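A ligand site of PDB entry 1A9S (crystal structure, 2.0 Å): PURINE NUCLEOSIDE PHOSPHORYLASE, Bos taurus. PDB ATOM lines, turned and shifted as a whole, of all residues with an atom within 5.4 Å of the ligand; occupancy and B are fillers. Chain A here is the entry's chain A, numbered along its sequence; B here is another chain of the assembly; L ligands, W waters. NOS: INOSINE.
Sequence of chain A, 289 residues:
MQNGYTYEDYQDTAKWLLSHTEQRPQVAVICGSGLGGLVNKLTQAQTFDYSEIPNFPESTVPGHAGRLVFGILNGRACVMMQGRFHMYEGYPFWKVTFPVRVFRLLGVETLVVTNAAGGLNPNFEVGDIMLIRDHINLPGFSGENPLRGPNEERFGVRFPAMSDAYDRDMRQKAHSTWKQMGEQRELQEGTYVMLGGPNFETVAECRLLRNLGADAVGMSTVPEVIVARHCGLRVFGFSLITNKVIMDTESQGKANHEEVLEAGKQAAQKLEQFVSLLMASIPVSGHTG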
ATOM      1  N   SER A  33       8.930   8.899   8.630  1.00  0.00           N
ATOM      2  CA  SER A  33       9.515   8.467   7.355  1.00  0.00           C
ATOM      3  C   SER A  33       8.494   8.432   6.225  1.00  0.00           C
ATOM      4  O   SER A  33       7.440   7.805   6.345  1.00  0.00           O
ATOM      5  CB  SER A  33      10.151   7.074   7.513  1.00  0.00           C
ATOM      6  OG  SER A  33      11.219   7.081   8.439  1.00  0.00           O
ATOM      7  N   HIS A  64      13.953  12.285   6.193  1.00  0.00           N
ATOM      8  CA  HIS A  64      13.775  13.264   7.267  1.00  0.00           C
ATOM      9  C   HIS A  64      14.577  14.507   6.879  1.00  0.00           C
ATOM     10  O   HIS A  64      15.779  14.583   7.133  1.00  0.00           O
ATOM     11  CB  HIS A  64      14.247  12.675   8.600  1.00  0.00           C
ATOM     12  CG  HIS A  64      13.462  11.483   9.035  1.00  0.00           C
ATOM     13  ND1 HIS A  64      13.667  10.226   8.505  1.00  0.00           N
ATOM     14  CD2 HIS A  64      12.447  11.346   9.916  1.00  0.00           C
ATOM     15  CE1 HIS A  64      12.806   9.374   9.034  1.00  0.00           C
ATOM     16  NE2 HIS A  64      12.049  10.033   9.895  1.00  0.00           N
ATOM     17  N   HIS A  86      15.736   9.872  16.208  1.00  0.00           N
ATOM     18  CA  HIS A  86      15.593   8.508  16.704  1.00  0.00           C
ATOM     19  C   HIS A  86      16.773   8.138  17.575  1.00  0.00           C
ATOM     20  O   HIS A  86      17.880   8.662  17.406  1.00  0.00           O
ATOM     21  CB  HIS A  86      15.517   7.525  15.537  1.00  0.00           C
ATOM     22  CG  HIS A  86      14.565   7.919  14.457  1.00  0.00           C
ATOM     23  ND1 HIS A  86      14.854   8.872  13.509  1.00  0.00           N
ATOM     24  CD2 HIS A  86      13.327   7.447  14.152  1.00  0.00           C
ATOM     25  CE1 HIS A  86      13.852   8.970  12.651  1.00  0.00           C
ATOM     26  NE2 HIS A  86      12.916   8.116  13.022  1.00  0.00           N
ATOM     27  N   TYR A  88      18.324   5.274  17.518  1.00  0.00           N
ATOM     28  CA  TYR A  88      19.334   4.561  16.738  1.00  0.00           C
ATOM     29  C   TYR A  88      20.367   5.458  16.045  1.00  0.00           C
ATOM     30  O   TYR A  88      21.364   4.965  15.545  1.00  0.00           O
ATOM     31  CB  TYR A  88      18.704   3.589  15.719  1.00  0.00           C
ATOM     32  CG  TYR A  88      17.824   4.223  14.658  1.00  0.00           C
ATOM     33  CD1 TYR A  88      18.368   5.006  13.644  1.00  0.00           C
ATOM     34  CD2 TYR A  88      16.445   4.045  14.679  1.00  0.00           C
ATOM     35  CE1 TYR A  88      17.559   5.603  12.681  1.00  0.00           C
ATOM     36  CE2 TYR A  88      15.630   4.632  13.723  1.00  0.00           C
ATOM     37  CZ  TYR A  88      16.192   5.416  12.732  1.00  0.00           C
ATOM     38  OH  TYR A  88      15.371   5.991  11.781  1.00  0.00           O
ATOM     39  N   ALA A 116       6.099   5.559  10.251  1.00  0.00           N
ATOM     40  CA  ALA A 116       6.006   4.465   9.284  1.00  0.00           C
ATOM     41  C   ALA A 116       6.210   3.248  10.173  1.00  0.00           C
ATOM     42  O   ALA A 116       7.146   3.225  10.977  1.00  0.00           O
ATOM     43  CB  ALA A 116       7.126   4.579   8.256  1.00  0.00           C
ATOM     44  N   ALA A 117       5.372   2.232  10.027  1.00  0.00           N
ATOM     45  CA  ALA A 117       5.487   1.037  10.857  1.00  0.00           C
ATOM     46  C   ALA A 117       5.276  -0.270  10.124  1.00  0.00           C
ATOM     47  O   ALA A 117       4.620  -0.317   9.076  1.00  0.00           O
ATOM     48  CB  ALA A 117       4.516   1.127  12.025  1.00  0.00           C
ATOM     49  N   GLY A 118       5.832  -1.345  10.687  1.00  0.00           N
ATOM     50  CA  GLY A 118       5.676  -2.661  10.102  1.00  0.00           C
ATOM     51  C   GLY A 118       4.408  -3.248  10.685  1.00  0.00           C
ATOM     52  O   GLY A 118       4.143  -3.100  11.874  1.00  0.00           O
ATOM     53  N   TYR A 192       0.814   0.270  19.147  1.00  0.00           N
ATOM     54  CA  TYR A 192       2.100   0.478  18.519  1.00  0.00           C
ATOM     55  C   TYR A 192       3.187   0.063  19.506  1.00  0.00           C
ATOM     56  O   TYR A 192       3.136   0.428  20.678  1.00  0.00           O
ATOM     57  CB  TYR A 192       2.247   1.949  18.143  1.00  0.00           C
ATOM     58  CG  TYR A 192       3.598   2.333  17.594  1.00  0.00           C
ATOM     59  CD1 TYR A 192       3.886   2.203  16.245  1.00  0.00           C
ATOM     60  CD2 TYR A 192       4.593   2.839  18.438  1.00  0.00           C
ATOM     61  CE1 TYR A 192       5.120   2.572  15.740  1.00  0.00           C
ATOM     62  CE2 TYR A 192       5.819   3.207  17.939  1.00  0.00           C
ATOM     63  CZ  TYR A 192       6.079   3.073  16.587  1.00  0.00           C
ATOM     64  OH  TYR A 192       7.318   3.433  16.104  1.00  0.00           O
ATOM     65  N   LEU A 195      10.781  -0.377  19.554  1.00  0.00           N
ATOM     66  CA  LEU A 195      12.033  -1.043  19.884  1.00  0.00           C
ATOM     67  C   LEU A 195      13.125  -0.105  19.385  1.00  0.00           C
ATOM     68  O   LEU A 195      12.826   0.834  18.650  1.00  0.00           O
ATOM     69  CB  LEU A 195      12.114  -2.441  19.256  1.00  0.00           C
ATOM     70  CG  LEU A 195      11.457  -2.790  17.930  1.00  0.00           C
ATOM     71  CD1 LEU A 195      12.101  -2.012  16.797  1.00  0.00           C
ATOM     72  CD2 LEU A 195      11.584  -4.308  17.706  1.00  0.00           C
ATOM     73  N   PHE A 200      16.233  -4.421  11.124  1.00  0.00           N
ATOM     74  CA  PHE A 200      14.856  -4.867  11.068  1.00  0.00           C
ATOM     75  C   PHE A 200      14.742  -6.158  11.870  1.00  0.00           C
ATOM     76  O   PHE A 200      15.731  -6.859  12.092  1.00  0.00           O
ATOM     77  CB  PHE A 200      14.387  -5.040   9.621  1.00  0.00           C
ATOM     78  CG  PHE A 200      14.066  -3.742   8.923  1.00  0.00           C
ATOM     79  CD1 PHE A 200      12.955  -2.995   9.295  1.00  0.00           C
ATOM     80  CD2 PHE A 200      14.856  -3.282   7.883  1.00  0.00           C
ATOM     81  CE1 PHE A 200      12.634  -1.809   8.641  1.00  0.00           C
ATOM     82  CE2 PHE A 200      14.551  -2.095   7.217  1.00  0.00           C
ATOM     83  CZ  PHE A 200      13.433  -1.359   7.595  1.00  0.00           C
ATOM     84  N   GLU A 201      13.519  -6.502  12.263  1.00  0.00           N
ATOM     85  CA  GLU A 201      13.252  -7.669  13.089  1.00  0.00           C
ATOM     86  C   GLU A 201      13.439  -9.035  12.438  1.00  0.00           C
ATOM     87  O   GLU A 201      13.336  -9.194  11.223  1.00  0.00           O
ATOM     88  CB  GLU A 201      11.832  -7.579  13.667  1.00  0.00           C
ATOM     89  CG  GLU A 201      11.496  -6.317  14.468  1.00  0.00           C
ATOM     90  CD  GLU A 201      11.355  -5.053  13.602  1.00  0.00           C
ATOM     91  OE1 GLU A 201      10.795  -5.137  12.491  1.00  0.00           O
ATOM     92  OE2 GLU A 201      11.796  -3.971  14.036  1.00  0.00           O
ATOM     93  N   VAL A 217       4.947  -2.360  14.559  1.00  0.00           N
ATOM     94  CA  VAL A 217       6.243  -2.165  15.192  1.00  0.00           C
ATOM     95  C   VAL A 217       7.006  -1.008  14.546  1.00  0.00           C
ATOM     96  O   VAL A 217       6.964  -0.808  13.327  1.00  0.00           O
ATOM     97  CB  VAL A 217       7.074  -3.489  15.139  1.00  0.00           C
ATOM     98  CG1 VAL A 217       7.122  -4.026  13.709  1.00  0.00           C
ATOM     99  CG2 VAL A 217       8.471  -3.280  15.691  1.00  0.00           C
ATOM    100  N   GLY A 218       7.699  -0.214  15.371  1.00  0.00           N
ATOM    101  CA  GLY A 218       8.450   0.917  14.851  1.00  0.00           C
ATOM    102  C   GLY A 218       9.579   1.294  15.774  1.00  0.00           C
ATOM    103  O   GLY A 218       9.697   0.725  16.863  1.00  0.00           O
ATOM    104  N   MET A 219      10.392   2.267  15.367  1.00  0.00           N
ATOM    105  CA  MET A 219      11.552   2.713  16.133  1.00  0.00           C
ATOM    106  C   MET A 219      11.482   4.158  16.622  1.00  0.00           C
ATOM    107  O   MET A 219      12.517   4.847  16.681  1.00  0.00           O
ATOM    108  CB  MET A 219      12.813   2.535  15.277  1.00  0.00           C
ATOM    109  CG  MET A 219      13.008   1.116  14.739  1.00  0.00           C
ATOM    110  SD  MET A 219      14.295   1.045  13.485  1.00  0.00           S
ATOM    111  CE  MET A 219      14.107  -0.646  12.857  1.00  0.00           C
ATOM    112  N   SER A 220      10.296   4.636  16.966  1.00  0.00           N
ATOM    113  CA  SER A 220      10.165   6.025  17.417  1.00  0.00           C
ATOM    114  C   SER A 220       8.812   6.281  18.060  1.00  0.00           C
ATOM    115  O   SER A 220       8.142   5.362  18.542  1.00  0.00           O
ATOM    116  CB  SER A 220      10.271   6.956  16.206  1.00  0.00           C
ATOM    117  OG  SER A 220       9.053   6.895  15.453  1.00  0.00           O
ATOM    118  N   THR A 242       3.780   0.392   6.314  1.00  0.00           N
ATOM    119  CA  THR A 242       4.617   0.379   5.122  1.00  0.00           C
ATOM    120  C   THR A 242       4.979  -1.001   4.589  1.00  0.00           C
ATOM    121  O   THR A 242       5.393  -1.124   3.445  1.00  0.00           O
ATOM    122  CB  THR A 242       5.912   1.223   5.323  1.00  0.00           C
ATOM    123  OG1 THR A 242       6.583   0.804   6.514  1.00  0.00           O
ATOM    124  CG2 THR A 242       5.565   2.710   5.442  1.00  0.00           C
ATOM    125  N   ASN A 243       4.773  -2.040   5.385  1.00  0.00           N
ATOM    126  CA  ASN A 243       5.091  -3.378   4.949  1.00  0.00           C
ATOM    127  C   ASN A 243       4.551  -4.410   5.909  1.00  0.00           C
ATOM    128  O   ASN A 243       4.237  -4.094   7.051  1.00  0.00           O
ATOM    129  CB  ASN A 243       6.611  -3.564   4.847  1.00  0.00           C
ATOM    130  CG  ASN A 243       7.320  -3.381   6.193  1.00  0.00           C
ATOM    131  OD1 ASN A 243       7.488  -2.261   6.663  1.00  0.00           O
ATOM    132  ND2 ASN A 243       7.721  -4.486   6.816  1.00  0.00           N
ATOM    133  N   VAL A 245       5.444  -7.536   8.005  1.00  0.00           N
ATOM    134  CA  VAL A 245       6.676  -8.140   8.515  1.00  0.00           C
ATOM    135  C   VAL A 245       6.700  -9.638   8.231  1.00  0.00           C
ATOM    136  O   VAL A 245       5.650 -10.300   8.222  1.00  0.00           O
ATOM    137  CB  VAL A 245       6.855  -7.872  10.035  1.00  0.00           C
ATOM    138  CG1 VAL A 245       6.898  -6.386  10.303  1.00  0.00           C
ATOM    139  CG2 VAL A 245       5.748  -8.530  10.838  1.00  0.00           C
ATOM    140  N   ALA A 255      12.727  -6.849   4.578  1.00  0.00           N
ATOM    141  CA  ALA A 255      12.480  -5.423   4.748  1.00  0.00           C
ATOM    142  C   ALA A 255      13.648  -4.522   4.369  1.00  0.00           C
ATOM    143  O   ALA A 255      14.819  -4.897   4.505  1.00  0.00           O
ATOM    144  CB  ALA A 255      12.043  -5.131   6.182  1.00  0.00           C
ATOM    145  N   ASN A 256      13.319  -3.314   3.900  1.00  0.00           N
ATOM    146  CA  ASN A 256      14.301  -2.311   3.485  1.00  0.00           C
ATOM    147  C   ASN A 256      13.691  -0.914   3.600  1.00  0.00           C
ATOM    148  O   ASN A 256      12.480  -0.734   3.443  1.00  0.00           O
ATOM    149  CB  ASN A 256      14.756  -2.571   2.047  1.00  0.00           C
ATOM    150  CG  ASN A 256      13.604  -2.535   1.056  1.00  0.00           C
ATOM    151  OD1 ASN A 256      13.341  -1.505   0.430  1.00  0.00           O
ATOM    152  ND2 ASN A 256      12.913  -3.655   0.914  1.00  0.00           N
ATOM    153  N   HIS A 257      14.527   0.077   3.866  1.00  0.00           N
ATOM    154  CA  HIS A 257      14.079   1.461   4.020  1.00  0.00           C
ATOM    155  C   HIS A 257      13.458   2.041   2.742  1.00  0.00           C
ATOM    156  O   HIS A 257      12.607   2.938   2.822  1.00  0.00           O
ATOM    157  CB  HIS A 257      15.247   2.342   4.487  1.00  0.00           C
ATOM    158  CG  HIS A 257      14.839   3.720   4.929  1.00  0.00           C
ATOM    159  ND1 HIS A 257      13.754   3.950   5.756  1.00  0.00           N
ATOM    160  CD2 HIS A 257      15.386   4.929   4.683  1.00  0.00           C
ATOM    161  CE1 HIS A 257      13.650   5.249   5.986  1.00  0.00           C
ATOM    162  NE2 HIS A 257      14.628   5.866   5.351  1.00  0.00           N
ATOM    163  N   VAL A 260       9.774   1.512   2.470  1.00  0.00           N
ATOM    164  CA  VAL A 260       9.138   2.413   3.427  1.00  0.00           C
ATOM    165  C   VAL A 260       8.878   3.785   2.817  1.00  0.00           C
ATOM    166  O   VAL A 260       7.768   4.329   2.931  1.00  0.00           O
ATOM    167  CB  VAL A 260       9.996   2.544   4.708  1.00  0.00           C
ATOM    168  CG1 VAL A 260       9.445   3.638   5.612  1.00  0.00           C
ATOM    169  CG2 VAL A 260      10.024   1.212   5.437  1.00  0.00           C
ATOM    170  N   PHE B 159      19.622   0.573   7.264  1.00  0.00           N
ATOM    171  CA  PHE B 159      18.601  -0.327   7.795  1.00  0.00           C
ATOM    172  C   PHE B 159      18.732  -1.764   7.270  1.00  0.00           C
ATOM    173  O   PHE B 159      17.967  -2.192   6.405  1.00  0.00           O
ATOM    174  CB  PHE B 159      17.208   0.213   7.443  1.00  0.00           C
ATOM    175  CG  PHE B 159      16.915   1.579   8.011  1.00  0.00           C
ATOM    176  CD1 PHE B 159      16.708   1.748   9.371  1.00  0.00           C
ATOM    177  CD2 PHE B 159      16.830   2.686   7.187  1.00  0.00           C
ATOM    178  CE1 PHE B 159      16.417   3.005   9.906  1.00  0.00           C
ATOM    179  CE2 PHE B 159      16.542   3.945   7.693  1.00  0.00           C
ATOM    180  CZ  PHE B 159      16.335   4.114   9.053  1.00  0.00           C
HETATM  181  N9  NOS L   1       9.744   1.179  10.233  1.00  0.00           N
HETATM  182  C4  NOS L   1       9.970  -0.007  10.898  1.00  0.00           C
HETATM  183  N3  NOS L   1      10.615  -0.238  12.074  1.00  0.00           N
HETATM  184  C2  NOS L   1      10.642  -1.525  12.378  1.00  0.00           C
HETATM  185  N1  NOS L   1      10.100  -2.505  11.596  1.00  0.00           N
HETATM  186  C6  NOS L   1       9.448  -2.294  10.390  1.00  0.00           C
HETATM  187  O6  NOS L   1       9.047  -3.262   9.737  1.00  0.00           O
HETATM  188  C5  NOS L   1       9.395  -0.938  10.050  1.00  0.00           C
HETATM  189  N7  NOS L   1       8.845  -0.336   8.945  1.00  0.00           N
HETATM  190  C8  NOS L   1       9.064   1.003   9.069  1.00  0.00           C
HETATM  191  C5' NOS L   1      12.849   2.147   8.804  1.00  0.00           C
HETATM  192  O5' NOS L   1      12.333   2.227   7.457  1.00  0.00           O
HETATM  193  C4' NOS L   1      12.276   3.323   9.568  1.00  0.00           C
HETATM  194  O4' NOS L   1      10.831   3.234   9.459  1.00  0.00           O
HETATM  195  C1' NOS L   1      10.285   2.576  10.621  1.00  0.00           C
HETATM  196  C2' NOS L   1      11.398   2.674  11.700  1.00  0.00           C
HETATM  197  O2' NOS L   1      10.940   3.468  12.828  1.00  0.00           O
HETATM  198  C3' NOS L   1      12.642   3.362  11.041  1.00  0.00           C
HETATM  199  O3' NOS L   1      12.866   4.729  11.544  1.00  0.00           O
HETATM  200  O   HOH W   1      10.714  -6.225  10.016  1.00  0.00           O
HETATM  201  O   HOH W   2       7.854   3.807  13.531  1.00  0.00           O
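The side-chain hydroxyl (OH) of Tyr 88 is in hydrogen-bond range of an oxygen (O3') of the ligand, at 2.8 Å. The backbone NH of Met 219 sits at hydrogen-bond distance from an oxygen (O2') of the ligand (2.9 Å). O5' of the ligand is in hydrogen-bond range of ND1 of His 257. N1 of the ligand is in hydrogen-bond range of OE1 of Glu 201. A nitrogen (N7) of the ligand sits close to the side-chain amide oxygen (OD1) of Asn 243 (3.3 Å).
OH of Tyr 192 lies within hydrogen-bond range of N of Met 219, at 3.4 Å. The side-chain hydroxyl (OH) of Tyr 88 lies close to a ring nitrogen (ND1) of His 86 (3.4 Å). The backbone carbonyl oxygen (O) of Gly 218 is in hydrogen-bond range of the backbone NH (N) of Leu 195 (3.1 Å). N of Val 217 is in hydrogen-bond range of O of Gly 118, 2.9 Å away. The side-chain hydroxyl (OG) of Ser 33 lies close to a ring nitrogen (NE2) of His 64 (3.4 Å). OD1 of Asn 243 is in hydrogen-bond range of OG1 of Thr 242, at 3.2 Å. The backbone NH of Thr 242 is in hydrogen-bond range of the backbone carbonyl oxygen of Ala 117 (3.0 Å).
The backbone carbonyl oxygen (O) of Ala 116 sits close to a nitrogen (N9) of the ligand, 3.4 Å away. Merely in contact with the ligand: Ser 33 (3.999 Å), His 86 (3.7 Å), Ala 117 (3.8 Å), Gly 118 (3.4 Å), Phe 200 (3.6 Å), Val 217 (3.9 Å), Gly 218 (3.7 Å), Thr 242 (3.5 Å), Val 245 (3.8 Å), Val 260 (3.2 Å) and Phe 159 of chain B (3.8 Å). Hydrophobic or aromatic side chains within 4 Å of the ligand: His 86, Tyr 88, Phe 200, Val 217, Met 219, Val 245, His 257, Val 260 and Phe 159 of chain B. Of the 23 residues printed, 17 come within 4 Å of the ligand.
Water W2 lies within hydrogen-bond range of OH of Tyr 192 (2.7 Å), O of Ala 116 (2.7 Å), O2' of the ligand (3.2 Å) and N of Met 219 (3.5 Å). Water W1 lies within hydrogen-bond range of the side-chain carboxylate of Glu 201 and an oxygen (O6) of the ligand.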
